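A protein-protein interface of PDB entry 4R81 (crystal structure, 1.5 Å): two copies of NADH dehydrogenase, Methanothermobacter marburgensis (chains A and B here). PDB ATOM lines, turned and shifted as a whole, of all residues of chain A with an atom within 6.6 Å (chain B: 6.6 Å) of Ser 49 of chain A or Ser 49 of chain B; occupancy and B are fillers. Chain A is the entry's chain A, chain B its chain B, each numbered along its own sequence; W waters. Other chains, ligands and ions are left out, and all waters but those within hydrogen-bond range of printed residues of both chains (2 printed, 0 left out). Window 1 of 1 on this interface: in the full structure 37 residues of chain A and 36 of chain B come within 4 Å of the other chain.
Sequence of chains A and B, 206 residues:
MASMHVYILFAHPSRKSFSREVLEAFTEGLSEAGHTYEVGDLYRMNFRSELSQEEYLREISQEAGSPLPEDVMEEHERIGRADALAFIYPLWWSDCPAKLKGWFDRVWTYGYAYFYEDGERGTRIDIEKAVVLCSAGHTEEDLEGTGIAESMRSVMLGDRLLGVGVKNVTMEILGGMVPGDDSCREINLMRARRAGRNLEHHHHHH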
ATOM      1  N   TYR A  43       4.513  23.194 -17.750  1.00  0.00           N
ATOM      2  CA  TYR A  43       4.195  24.623 -17.702  1.00  0.00           C
ATOM      3  C   TYR A  43       3.314  24.962 -16.503  1.00  0.00           C
ATOM      4  O   TYR A  43       3.574  25.944 -15.798  1.00  0.00           O
ATOM      5  CB  TYR A  43       3.532  25.089 -18.997  1.00  0.00           C
ATOM      6  CG  TYR A  43       4.488  25.592 -20.058  1.00  0.00           C
ATOM      7  CD1 TYR A  43       4.805  26.947 -20.154  1.00  0.00           C
ATOM      8  CD2 TYR A  43       5.057  24.720 -20.975  1.00  0.00           C
ATOM      9  CE1 TYR A  43       5.669  27.414 -21.129  1.00  0.00           C
ATOM     10  CE2 TYR A  43       5.923  25.177 -21.956  1.00  0.00           C
ATOM     11  CZ  TYR A  43       6.213  26.529 -22.033  1.00  0.00           C
ATOM     12  OH  TYR A  43       7.062  26.997 -23.004  1.00  0.00           O
ATOM     13  N   ASN A  46       5.071  25.217 -13.232  1.00  0.00           N
ATOM     14  CA  ASN A  46       6.123  26.237 -13.164  1.00  0.00           C
ATOM     15  C   ASN A  46       7.510  25.595 -13.057  1.00  0.00           C
ATOM     16  O   ASN A  46       8.390  26.081 -12.345  1.00  0.00           O
ATOM     17  CB  ASN A  46       5.873  27.209 -12.004  1.00  0.00           C
ATOM     18  CG  ASN A  46       4.541  27.923 -12.121  1.00  0.00           C
ATOM     19  OD1 ASN A  46       3.616  27.681 -11.339  1.00  0.00           O
ATOM     20  ND2 ASN A  46       4.436  28.813 -13.102  1.00  0.00           N
ATOM     21  N   PHE A  47       7.699  24.498 -13.781  1.00  0.00           N
ATOM     22  CA  PHE A  47       8.928  23.726 -13.676  1.00  0.00           C
ATOM     23  C   PHE A  47      10.131  24.523 -14.146  1.00  0.00           C
ATOM     24  O   PHE A  47      10.143  25.049 -15.261  1.00  0.00           O
ATOM     25  CB  PHE A  47       8.825  22.427 -14.468  1.00  0.00           C
ATOM     26  CG  PHE A  47      10.012  21.523 -14.295  1.00  0.00           C
ATOM     27  CD1 PHE A  47      10.135  20.734 -13.159  1.00  0.00           C
ATOM     28  CD2 PHE A  47      11.010  21.469 -15.259  1.00  0.00           C
ATOM     29  CE1 PHE A  47      11.230  19.898 -12.992  1.00  0.00           C
ATOM     30  CE2 PHE A  47      12.105  20.637 -15.098  1.00  0.00           C
ATOM     31  CZ  PHE A  47      12.216  19.853 -13.963  1.00  0.00           C
ATOM     32  N   ARG A  48      11.143  24.603 -13.289  1.00  0.00           N
ATOM     33  CA  ARG A  48      12.359  25.332 -13.608  1.00  0.00           C
ATOM     34  C   ARG A  48      13.140  24.535 -14.641  1.00  0.00           C
ATOM     35  O   ARG A  48      13.544  23.389 -14.397  1.00  0.00           O
ATOM     36  CB  ARG A  48      13.206  25.544 -12.351  1.00  0.00           C
ATOM     37  CG  ARG A  48      14.518  26.272 -12.605  1.00  0.00           C
ATOM     38  CD  ARG A  48      14.270  27.678 -13.102  1.00  0.00           C
ATOM     39  NE  ARG A  48      15.504  28.447 -13.190  1.00  0.00           N
ATOM     40  CZ  ARG A  48      15.567  29.717 -13.572  1.00  0.00           C
ATOM     41  NH1 ARG A  48      14.459  30.367 -13.896  1.00  0.00           N
ATOM     42  NH2 ARG A  48      16.738  30.332 -13.632  1.00  0.00           N
ATOM     43  N   SER A  49      13.355  25.124 -15.807  1.00  0.00           N
ATOM     44  CA  SER A  49      13.995  24.367 -16.873  1.00  0.00           C
ATOM     45  C   SER A  49      15.499  24.598 -16.991  1.00  0.00           C
ATOM     46  O   SER A  49      16.175  23.834 -17.662  1.00  0.00           O
ATOM     47  CB  SER A  49      13.288  24.602 -18.208  1.00  0.00           C
ATOM     48  OG  SER A  49      13.412  25.939 -18.613  1.00  0.00           O
ATOM     49  N   GLU A  50      16.032  25.629 -16.337  1.00  0.00           N
ATOM     50  CA  GLU A  50      17.469  25.915 -16.430  1.00  0.00           C
ATOM     51  C   GLU A  50      18.285  25.153 -15.403  1.00  0.00           C
ATOM     52  O   GLU A  50      18.074  25.323 -14.201  1.00  0.00           O
ATOM     53  CB  GLU A  50      17.758  27.405 -16.216  1.00  0.00           C
ATOM     54  CG  GLU A  50      17.462  28.297 -17.397  1.00  0.00           C
ATOM     55  CD  GLU A  50      16.060  28.852 -17.363  1.00  0.00           C
ATOM     56  OE1 GLU A  50      15.274  28.423 -16.482  1.00  0.00           O
ATOM     57  OE2 GLU A  50      15.750  29.722 -18.214  1.00  0.00           O
ATOM     58  N   LEU A  51      19.233  24.345 -15.869  1.00  0.00           N
ATOM     59  CA  LEU A  51      20.223  23.762 -14.969  1.00  0.00           C
ATOM     60  C   LEU A  51      21.029  24.908 -14.374  1.00  0.00           C
ATOM     61  O   LEU A  51      21.698  25.641 -15.108  1.00  0.00           O
ATOM     62  CB  LEU A  51      21.166  22.835 -15.729  1.00  0.00           C
ATOM     63  CG  LEU A  51      22.105  22.001 -14.856  1.00  0.00           C
ATOM     64  CD1 LEU A  51      21.307  20.925 -14.158  1.00  0.00           C
ATOM     65  CD2 LEU A  51      23.236  21.398 -15.683  1.00  0.00           C
ATOM     66  N   ALA A  98      11.919  24.068 -25.091  1.00  0.00           N
ATOM     67  CA  ALA A  98      12.948  24.301 -24.087  1.00  0.00           C
ATOM     68  C   ALA A  98      12.542  23.784 -22.713  1.00  0.00           C
ATOM     69  O   ALA A  98      13.391  23.282 -21.968  1.00  0.00           O
ATOM     70  CB  ALA A  98      13.285  25.779 -24.012  1.00  0.00           C
ATOM     71  N   LYS A  99      11.254  23.914 -22.380  1.00  0.00           N
ATOM     72  CA  LYS A  99      10.747  23.456 -21.085  1.00  0.00           C
ATOM     73  C   LYS A  99      11.017  21.963 -20.868  1.00  0.00           C
ATOM     74  O   LYS A  99      11.437  21.554 -19.781  1.00  0.00           O
ATOM     75  CB  LYS A  99       9.248  23.742 -20.942  1.00  0.00           C
ATOM     76  CG  LYS A  99       8.643  23.156 -19.679  1.00  0.00           C
ATOM     77  CD  LYS A  99       8.991  23.979 -18.445  1.00  0.00           C
ATOM     78  CE  LYS A  99       8.062  25.182 -18.294  1.00  0.00           C
ATOM     79  NZ  LYS A  99       8.550  26.159 -17.272  1.00  0.00           N
ATOM     80  N   LEU A 100      10.804  21.153 -21.907  1.00  0.00           N
ATOM     81  CA  LEU A 100      11.045  19.722 -21.791  1.00  0.00           C
ATOM     82  C   LEU A 100      12.534  19.407 -21.884  1.00  0.00           C
ATOM     83  O   LEU A 100      13.019  18.494 -21.211  1.00  0.00           O
ATOM     84  CB  LEU A 100      10.255  18.939 -22.854  1.00  0.00           C
ATOM     85  CG  LEU A 100      10.390  17.415 -22.858  1.00  0.00           C
ATOM     86  CD1 LEU A 100      10.017  16.833 -21.498  1.00  0.00           C
ATOM     87  CD2 LEU A 100       9.527  16.829 -23.967  1.00  0.00           C
ATOM     88  N   LYS A 101      13.260  20.148 -22.722  1.00  0.00           N
ATOM     89  CA  LYS A 101      14.705  19.950 -22.823  1.00  0.00           C
ATOM     90  C   LYS A 101      15.329  20.148 -21.453  1.00  0.00           C
ATOM     91  O   LYS A 101      16.215  19.387 -21.050  1.00  0.00           O
ATOM     92  CB  LYS A 101      15.340  20.920 -23.827  1.00  0.00           C
ATOM     93  CG  LYS A 101      16.869  20.823 -23.932  1.00  0.00           C
ATOM     94  CD  LYS A 101      17.328  19.376 -24.159  1.00  0.00           C
ATOM     95  CE  LYS A 101      18.759  19.281 -24.644  1.00  0.00           C
ATOM     96  NZ  LYS A 101      19.721  19.874 -23.675  1.00  0.00           N
ATOM     97  N   GLY A 102      14.839  21.152 -20.729  1.00  0.00           N
ATOM     98  CA  GLY A 102      15.370  21.464 -19.417  1.00  0.00           C
ATOM     99  C   GLY A 102      15.032  20.398 -18.401  1.00  0.00           C
ATOM    100  O   GLY A 102      15.785  20.186 -17.449  1.00  0.00           O
ATOM    101  N   TRP A 103      13.907  19.716 -18.611  1.00  0.00           N
ATOM    102  CA  TRP A 103      13.550  18.581 -17.779  1.00  0.00           C
ATOM    103  C   TRP A 103      14.620  17.493 -17.916  1.00  0.00           C
ATOM    104  O   TRP A 103      15.092  16.964 -16.915  1.00  0.00           O
ATOM    105  CB  TRP A 103      12.171  18.051 -18.170  1.00  0.00           C
ATOM    106  CG  TRP A 103      11.616  16.991 -17.268  1.00  0.00           C
ATOM    107  CD1 TRP A 103      10.823  17.184 -16.175  1.00  0.00           C
ATOM    108  CD2 TRP A 103      11.780  15.566 -17.397  1.00  0.00           C
ATOM    109  NE1 TRP A 103      10.487  15.975 -15.610  1.00  0.00           N
ATOM    110  CE2 TRP A 103      11.058  14.966 -16.341  1.00  0.00           C
ATOM    111  CE3 TRP A 103      12.459  14.741 -18.310  1.00  0.00           C
ATOM    112  CZ2 TRP A 103      11.006  13.579 -16.162  1.00  0.00           C
ATOM    113  CZ3 TRP A 103      12.407  13.362 -18.130  1.00  0.00           C
ATOM    114  CH2 TRP A 103      11.686  12.799 -17.063  1.00  0.00           C
ATOM    115  N   ASP A 105      17.773  17.970 -18.890  1.00  0.00           N
ATOM    116  CA  ASP A 105      19.015  18.536 -18.344  1.00  0.00           C
ATOM    117  C   ASP A 105      19.070  18.388 -16.824  1.00  0.00           C
ATOM    118  O   ASP A 105      20.113  18.055 -16.256  1.00  0.00           O
ATOM    119  CB  ASP A 105      19.156  20.031 -18.674  1.00  0.00           C
ATOM    120  CG  ASP A 105      19.270  20.319 -20.165  1.00  0.00           C
ATOM    121  OD1 ASP A 105      19.547  19.392 -20.955  1.00  0.00           O
ATOM    122  OD2 ASP A 105      19.085  21.503 -20.539  1.00  0.00           O
ATOM    123  N   ARG A 106      17.931  18.636 -16.178  1.00  0.00           N
ATOM    124  CA  ARG A 106      17.857  18.695 -14.721  1.00  0.00           C
ATOM    125  C   ARG A 106      17.474  17.382 -14.039  1.00  0.00           C
ATOM    126  O   ARG A 106      17.851  17.140 -12.887  1.00  0.00           O
ATOM    127  CB  ARG A 106      16.879  19.798 -14.293  1.00  0.00           C
ATOM    128  CG  ARG A 106      17.273  21.201 -14.754  1.00  0.00           C
ATOM    129  CD  ARG A 106      16.433  22.267 -14.060  1.00  0.00           C
ATOM    130  NE  ARG A 106      16.595  22.178 -12.612  1.00  0.00           N
ATOM    131  CZ  ARG A 106      15.605  22.014 -11.737  1.00  0.00           C
ATOM    132  NH1 ARG A 106      14.347  21.959 -12.146  1.00  0.00           N
ATOM    133  NH2 ARG A 106      15.883  21.920 -10.442  1.00  0.00           N
ATOM    134  N   TYR B  43      22.561  33.093 -19.678  1.00  0.00           N
ATOM    135  CA  TYR B  43      22.366  32.922 -18.242  1.00  0.00           C
ATOM    136  C   TYR B  43      22.566  34.227 -17.470  1.00  0.00           C
ATOM    137  O   TYR B  43      21.799  34.543 -16.561  1.00  0.00           O
ATOM    138  CB  TYR B  43      23.305  31.860 -17.678  1.00  0.00           C
ATOM    139  CG  TYR B  43      22.789  30.435 -17.688  1.00  0.00           C
ATOM    140  CD1 TYR B  43      22.152  29.901 -16.577  1.00  0.00           C
ATOM    141  CD2 TYR B  43      22.983  29.604 -18.796  1.00  0.00           C
ATOM    142  CE1 TYR B  43      21.710  28.578 -16.567  1.00  0.00           C
ATOM    143  CE2 TYR B  43      22.544  28.283 -18.800  1.00  0.00           C
ATOM    144  CZ  TYR B  43      21.903  27.775 -17.686  1.00  0.00           C
ATOM    145  OH  TYR B  43      21.481  26.457 -17.688  1.00  0.00           O
ATOM    146  N   ASN B  46      19.824  36.636 -17.643  1.00  0.00           N
ATOM    147  CA  ASN B  46      18.568  36.071 -17.152  1.00  0.00           C
ATOM    148  C   ASN B  46      17.514  35.986 -18.255  1.00  0.00           C
ATOM    149  O   ASN B  46      16.332  36.256 -18.030  1.00  0.00           O
ATOM    150  CB  ASN B  46      18.032  36.854 -15.957  1.00  0.00           C
ATOM    151  CG  ASN B  46      17.604  35.953 -14.841  1.00  0.00           C
ATOM    152  OD1 ASN B  46      16.711  35.126 -15.015  1.00  0.00           O
ATOM    153  ND2 ASN B  46      18.246  36.093 -13.686  1.00  0.00           N
ATOM    154  N   PHE B  47      17.965  35.598 -19.446  1.00  0.00           N
ATOM    155  CA  PHE B  47      17.105  35.516 -20.618  1.00  0.00           C
ATOM    156  C   PHE B  47      15.982  34.503 -20.390  1.00  0.00           C
ATOM    157  O   PHE B  47      16.235  33.357 -20.002  1.00  0.00           O
ATOM    158  CB  PHE B  47      17.927  35.147 -21.862  1.00  0.00           C
ATOM    159  CG  PHE B  47      17.109  35.079 -23.124  1.00  0.00           C
ATOM    160  CD1 PHE B  47      16.798  36.239 -23.825  1.00  0.00           C
ATOM    161  CD2 PHE B  47      16.630  33.859 -23.601  1.00  0.00           C
ATOM    162  CE1 PHE B  47      16.024  36.187 -24.976  1.00  0.00           C
ATOM    163  CE2 PHE B  47      15.857  33.803 -24.752  1.00  0.00           C
ATOM    164  CZ  PHE B  47      15.559  34.965 -25.441  1.00  0.00           C
ATOM    165  N   ARG B  48      14.739  34.915 -20.623  1.00  0.00           N
ATOM    166  CA  ARG B  48      13.616  33.994 -20.435  1.00  0.00           C
ATOM    167  C   ARG B  48      13.562  32.983 -21.574  1.00  0.00           C
ATOM    168  O   ARG B  48      13.469  33.357 -22.745  1.00  0.00           O
ATOM    169  CB  ARG B  48      12.274  34.716 -20.344  1.00  0.00           C
ATOM    170  CG  ARG B  48      11.120  33.714 -20.370  1.00  0.00           C
ATOM    171  CD  ARG B  48       9.826  34.278 -19.839  1.00  0.00           C
ATOM    172  NE  ARG B  48       9.345  35.407 -20.629  1.00  0.00           N
ATOM    173  CZ  ARG B  48       8.593  35.297 -21.722  1.00  0.00           C
ATOM    174  NH1 ARG B  48       8.237  34.104 -22.178  1.00  0.00           N
ATOM    175  NH2 ARG B  48       8.203  36.387 -22.367  1.00  0.00           N
ATOM    176  N   SER B  49      13.609  31.701 -21.234  1.00  0.00           N
ATOM    177  CA  SER B  49      13.741  30.684 -22.266  1.00  0.00           C
ATOM    178  C   SER B  49      12.434  30.033 -22.684  1.00  0.00           C
ATOM    179  O   SER B  49      12.378  29.405 -23.729  1.00  0.00           O
ATOM    180  CB  SER B  49      14.760  29.619 -21.856  1.00  0.00           C
ATOM    181  OG  SER B  49      14.378  28.988 -20.654  1.00  0.00           O
ATOM    182  N   GLU B  50      11.378  30.183 -21.888  1.00  0.00           N
ATOM    183  CA  GLU B  50      10.109  29.531 -22.228  1.00  0.00           C
ATOM    184  C   GLU B  50       9.171  30.395 -23.074  1.00  0.00           C
ATOM    185  O   GLU B  50       8.787  31.495 -22.672  1.00  0.00           O
ATOM    186  CB  GLU B  50       9.367  29.058 -20.976  1.00  0.00           C
ATOM    187  CG  GLU B  50      10.030  27.907 -20.259  1.00  0.00           C
ATOM    188  CD  GLU B  50      10.778  28.365 -19.036  1.00  0.00           C
ATOM    189  OE1 GLU B  50      11.161  29.562 -18.995  1.00  0.00           O
ATOM    190  OE2 GLU B  50      10.967  27.541 -18.113  1.00  0.00           O
ATOM    191  N   LEU B  51       8.791  29.879 -24.238  1.00  0.00           N
ATOM    192  CA  LEU B  51       7.775  30.522 -25.056  1.00  0.00           C
ATOM    193  C   LEU B  51       6.484  30.536 -24.243  1.00  0.00           C
ATOM    194  O   LEU B  51       6.044  29.492 -23.759  1.00  0.00           O
ATOM    195  CB  LEU B  51       7.555  29.726 -26.346  1.00  0.00           C
ATOM    196  CG  LEU B  51       6.679  30.363 -27.425  1.00  0.00           C
ATOM    197  CD1 LEU B  51       7.452  31.501 -28.055  1.00  0.00           C
ATOM    198  CD2 LEU B  51       6.306  29.323 -28.476  1.00  0.00           C
ATOM    199  N   ALA B  98      18.877  23.902 -22.422  1.00  0.00           N
ATOM    200  CA  ALA B  98      17.523  24.423 -22.552  1.00  0.00           C
ATOM    201  C   ALA B  98      17.498  25.936 -22.768  1.00  0.00           C
ATOM    202  O   ALA B  98      16.676  26.438 -23.523  1.00  0.00           O
ATOM    203  CB  ALA B  98      16.699  24.049 -21.341  1.00  0.00           C
ATOM    204  N   LYS B  99      18.411  26.653 -22.119  1.00  0.00           N
ATOM    205  CA  LYS B  99      18.440  28.111 -22.229  1.00  0.00           C
ATOM    206  C   LYS B  99      18.602  28.569 -23.678  1.00  0.00           C
ATOM    207  O   LYS B  99      17.927  29.498 -24.128  1.00  0.00           O
ATOM    208  CB  LYS B  99      19.564  28.680 -21.361  1.00  0.00           C
ATOM    209  CG  LYS B  99      19.690  30.191 -21.430  1.00  0.00           C
ATOM    210  CD  LYS B  99      18.574  30.860 -20.646  1.00  0.00           C
ATOM    211  CE  LYS B  99      19.024  31.193 -19.235  1.00  0.00           C
ATOM    212  NZ  LYS B  99      17.914  31.753 -18.401  1.00  0.00           N
ATOM    213  N   LEU B 100      19.497  27.913 -24.410  1.00  0.00           N
ATOM    214  CA  LEU B 100      19.731  28.246 -25.814  1.00  0.00           C
ATOM    215  C   LEU B 100      18.616  27.711 -26.709  1.00  0.00           C
ATOM    216  O   LEU B 100      18.234  28.366 -27.682  1.00  0.00           O
ATOM    217  CB  LEU B 100      21.105  27.755 -26.279  1.00  0.00           C
ATOM    218  CG  LEU B 100      21.456  28.013 -27.743  1.00  0.00           C
ATOM    219  CD1 LEU B 100      21.390  29.511 -28.072  1.00  0.00           C
ATOM    220  CD2 LEU B 100      22.828  27.452 -28.052  1.00  0.00           C
ATOM    221  N   LYS B 101      18.072  26.543 -26.377  1.00  0.00           N
ATOM    222  CA  LYS B 101      16.932  26.034 -27.138  1.00  0.00           C
ATOM    223  C   LYS B 101      15.789  27.043 -27.102  1.00  0.00           C
ATOM    224  O   LYS B 101      15.157  27.323 -28.121  1.00  0.00           O
ATOM    225  CB  LYS B 101      16.453  24.680 -26.602  1.00  0.00           C
ATOM    226  CG  LYS B 101      15.248  24.122 -27.347  1.00  0.00           C
ATOM    227  CD  LYS B 101      15.488  24.087 -28.863  1.00  0.00           C
ATOM    228  CE  LYS B 101      14.434  23.273 -29.601  1.00  0.00           C
ATOM    229  NZ  LYS B 101      13.017  23.621 -29.239  1.00  0.00           N
ATOM    230  N   GLY B 102      15.550  27.599 -25.919  1.00  0.00           N
ATOM    231  CA  GLY B 102      14.518  28.591 -25.723  1.00  0.00           C
ATOM    232  C   GLY B 102      14.741  29.856 -26.519  1.00  0.00           C
ATOM    233  O   GLY B 102      13.775  30.498 -26.958  1.00  0.00           O
ATOM    234  N   TRP B 103      16.010  30.227 -26.687  1.00  0.00           N
ATOM    235  CA  TRP B 103      16.363  31.362 -27.518  1.00  0.00           C
ATOM    236  C   TRP B 103      15.853  31.113 -28.940  1.00  0.00           C
ATOM    237  O   TRP B 103      15.216  31.973 -29.532  1.00  0.00           O
ATOM    238  CB  TRP B 103      17.878  31.603 -27.488  1.00  0.00           C
ATOM    239  CG  TRP B 103      18.334  32.838 -28.206  1.00  0.00           C
ATOM    240  CD1 TRP B 103      18.478  34.089 -27.670  1.00  0.00           C
ATOM    241  CD2 TRP B 103      18.726  32.947 -29.588  1.00  0.00           C
ATOM    242  NE1 TRP B 103      18.933  34.964 -28.627  1.00  0.00           N
ATOM    243  CE2 TRP B 103      19.085  34.297 -29.812  1.00  0.00           C
ATOM    244  CE3 TRP B 103      18.789  32.039 -30.655  1.00  0.00           C
ATOM    245  CZ2 TRP B 103      19.527  34.762 -31.058  1.00  0.00           C
ATOM    246  CZ3 TRP B 103      19.224  32.506 -31.900  1.00  0.00           C
ATOM    247  CH2 TRP B 103      19.589  33.858 -32.086  1.00  0.00           C
ATOM    248  N   ASP B 105      13.386  29.063 -29.801  1.00  0.00           N
ATOM    249  CA  ASP B 105      11.925  29.023 -29.721  1.00  0.00           C
ATOM    250  C   ASP B 105      11.322  30.426 -29.727  1.00  0.00           C
ATOM    251  O   ASP B 105      10.299  30.668 -30.370  1.00  0.00           O
ATOM    252  CB  ASP B 105      11.457  28.329 -28.439  1.00  0.00           C
ATOM    253  CG  ASP B 105      11.837  26.868 -28.373  1.00  0.00           C
ATOM    254  OD1 ASP B 105      12.226  26.276 -29.410  1.00  0.00           O
ATOM    255  OD2 ASP B 105      11.737  26.300 -27.260  1.00  0.00           O
ATOM    256  N   ARG B 106      11.964  31.346 -29.011  1.00  0.00           N
ATOM    257  CA  ARG B 106      11.408  32.677 -28.812  1.00  0.00           C
ATOM    258  C   ARG B 106      11.880  33.724 -29.811  1.00  0.00           C
ATOM    259  O   ARG B 106      11.173  34.696 -30.060  1.00  0.00           O
ATOM    260  CB  ARG B 106      11.708  33.177 -27.392  1.00  0.00           C
ATOM    261  CG  ARG B 106      11.096  32.309 -26.292  1.00  0.00           C
ATOM    262  CD  ARG B 106      11.249  32.967 -24.934  1.00  0.00           C
ATOM    263  NE  ARG B 106      10.537  34.241 -24.910  1.00  0.00           N
ATOM    264  CZ  ARG B 106      11.079  35.412 -24.586  1.00  0.00           C
ATOM    265  NH1 ARG B 106      12.348  35.484 -24.217  1.00  0.00           N
ATOM    266  NH2 ARG B 106      10.342  36.512 -24.620  1.00  0.00           N
HETATM  267  O   HOH W   1      13.596  31.141 -18.356  1.00  0.00           O
HETATM  268  O   HOH W   2      12.462  28.119 -16.184  1.00  0.00           O
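The backbone carbonyl oxygen of Phe 47 of chain A lies within hydrogen-bond range of the side-chain amino group of Lys 99 of chain A (2.8 Å).
NE of Arg 48 of chain A is in salt-bridge range of OE1 of Glu 50 of chain A (3.3 Å).
The side-chain amino group (NZ) of Lys 101 of chain A lies within salt-bridge range of the side-chain carboxylate (OD1) of Asp 105 of chain A.
The side-chain amino group (NZ) of Lys 99 of chain B sits at hydrogen-bond distance from the backbone carbonyl oxygen (O) of Phe 47 of chain B (2.8 Å).
The backbone carbonyl oxygen of Glu 50 of chain B sits at hydrogen-bond distance from the guanidinium group of Arg 48 of chain B, 2.7 Å away.
The side-chain amino group (NZ) of Lys 101 of chain B lies within salt-bridge range of the side-chain carboxylate (OD1) of Asp 105 of chain B (2.8 Å).
The side-chain hydroxyl (OH) of Tyr 43 of chain A lies within hydrogen-bond range of the backbone carbonyl oxygen (O) of Leu 51 of chain B, 2.8 Å away.
The side-chain carboxylate (OE2) of Glu 50 of chain B is in hydrogen-bond range of the side-chain hydroxyl (OG) of Ser 49 of chain A (3.0 Å).
The side-chain hydroxyl (OG) of Ser 49 of chain B sits at hydrogen-bond distance from the side-chain carboxylate (OE2) of Glu 50 of chain A (2.9 Å).
The side-chain carboxylate of Glu 50 of chain A lies within salt-bridge range of the side-chain amino group of Lys 99 of chain B (3.0 Å).
The backbone carbonyl oxygen (O) of Leu 51 of chain A is in hydrogen-bond range of the side-chain hydroxyl (OH) of Tyr 43 of chain B.
The side-chain carboxylate (OD2) of Asp 105 of chain B sits at hydrogen-bond distance from the backbone NH (N) of Ala 98 of chain A, 3.1 Å away.
NZ of Lys 99 of chain A lies within salt-bridge range of OE2 of Glu 50 of chain B (2.9 Å).
N of Ala 98 of chain B sits at hydrogen-bond distance from OD2 of Asp 105 of chain A, at 3.1 Å.
Hydrophobic or aromatic side chains of chain B within 4 Å of the printed part of chain A: Tyr 43 and Ala 98.
Printed residues of chain A that touch a printed residue of chain B: Tyr 43, Phe 47, Ser 49, Glu 50, Leu 51, Ala 98, Lys 99, Lys 101, Gly 102 and Asp 105.
Hydrophobic or aromatic side chains of chain A that line the printed part of chain B: Tyr 43 and Ala 98.
Among the printed residues, Asp or Glu carboxylates within 4 Å of a Lys or Arg side-chain nitrogen of the other chain: Glu 50 of chain A with Lys 99 of chain B (3.0 Å) and Lys 99 of chain A with Glu 50 of chain B (2.9 Å).
Among the printed residues, merely in contact across the chains: Tyr 43 of chain A with Glu 50 of chain B (3.7 Å), Phe 47 of chain A with Glu 50 of chain B (3.9 Å), Ser 49 of chain A with Ser 49 of chain B (3.8 Å), Ser 49 of chain A with Ala 98 of chain B (3.7 Å), Ala 98 of chain A with Ser 49 of chain B (3.7 Å), Ala 98 of chain A with Ala 98 of chain B (3.5 Å), Ala 98 of chain A with Lys 101 of chain B (3.99 Å), Ala 98 of chain A with Gly 102 of chain B (3.5 Å), Lys 101 of chain A with Ala 98 of chain B (3.9 Å) and Gly 102 of chain A with Ala 98 of chain B (3.5 Å).
Tyr 43 of chain A touches Glu 50 of chain B, but with the chains exchanged Glu 50 of chain A does not touch Tyr 43 of chain B (4.1 Å).
Ser 49 of chain A touches its own counterpart, Ser 49 of chain B.
Ala 98 of chain A touches Lys 101 of chain B, and with the chains exchanged Lys 101 of chain A touches Ala 98 of chain B.
Ala 98 of chain A touches Gly 102 of chain B, and with the chains exchanged Gly 102 of chain A touches Ala 98 of chain B.
Water W2 lies within hydrogen-bond range of OE2 of Glu 50 of chain B (2.5 Å), OE1 of Glu 50 of chain A (2.8 Å) and N of Ser 49 of chain A (3.1 Å).
Water W1 lies within hydrogen-bond range of OE2 of Glu 50 of chain A, N of Ser 49 of chain B and OE1 of Glu 50 of chain B.
Of chain B, only Ser 49, Glu 50 and Ala 98 come within 4 Å of Ser 49 of chain A.
Of chain A, only Ser 49 (3.8 Å), Glu 50 (2.9 Å) and Ala 98 (3.7 Å) come within 4 Å of Ser 49 of chain B.
Printed residues of chain B within 4 Å of Phe 47 of chain A: Glu 50.
Printed residues of chain B within 4 Å of Glu 50 of chain A: Ser 49 and Lys 99.
Printed residues of chain A within 4 Å of Leu 51 of chain B: Tyr 43.
Of the printed residues of chain B, Leu 51 of chain A touches Tyr 43 (2.7 Å).
Of the printed residues of chain B, Asp 105 of chain A touches Ala 98.
Asn 46 of chain B touches none of the printed residues of chain A.
The nearest residue of chain B that does not touch Ser 49 of chain A is Lys 99 of chain B (5.7 Å).
The nearest printed residue of chain B that does not touch Gly 102 of chain A is Lys 99 of chain B (6.6 Å).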
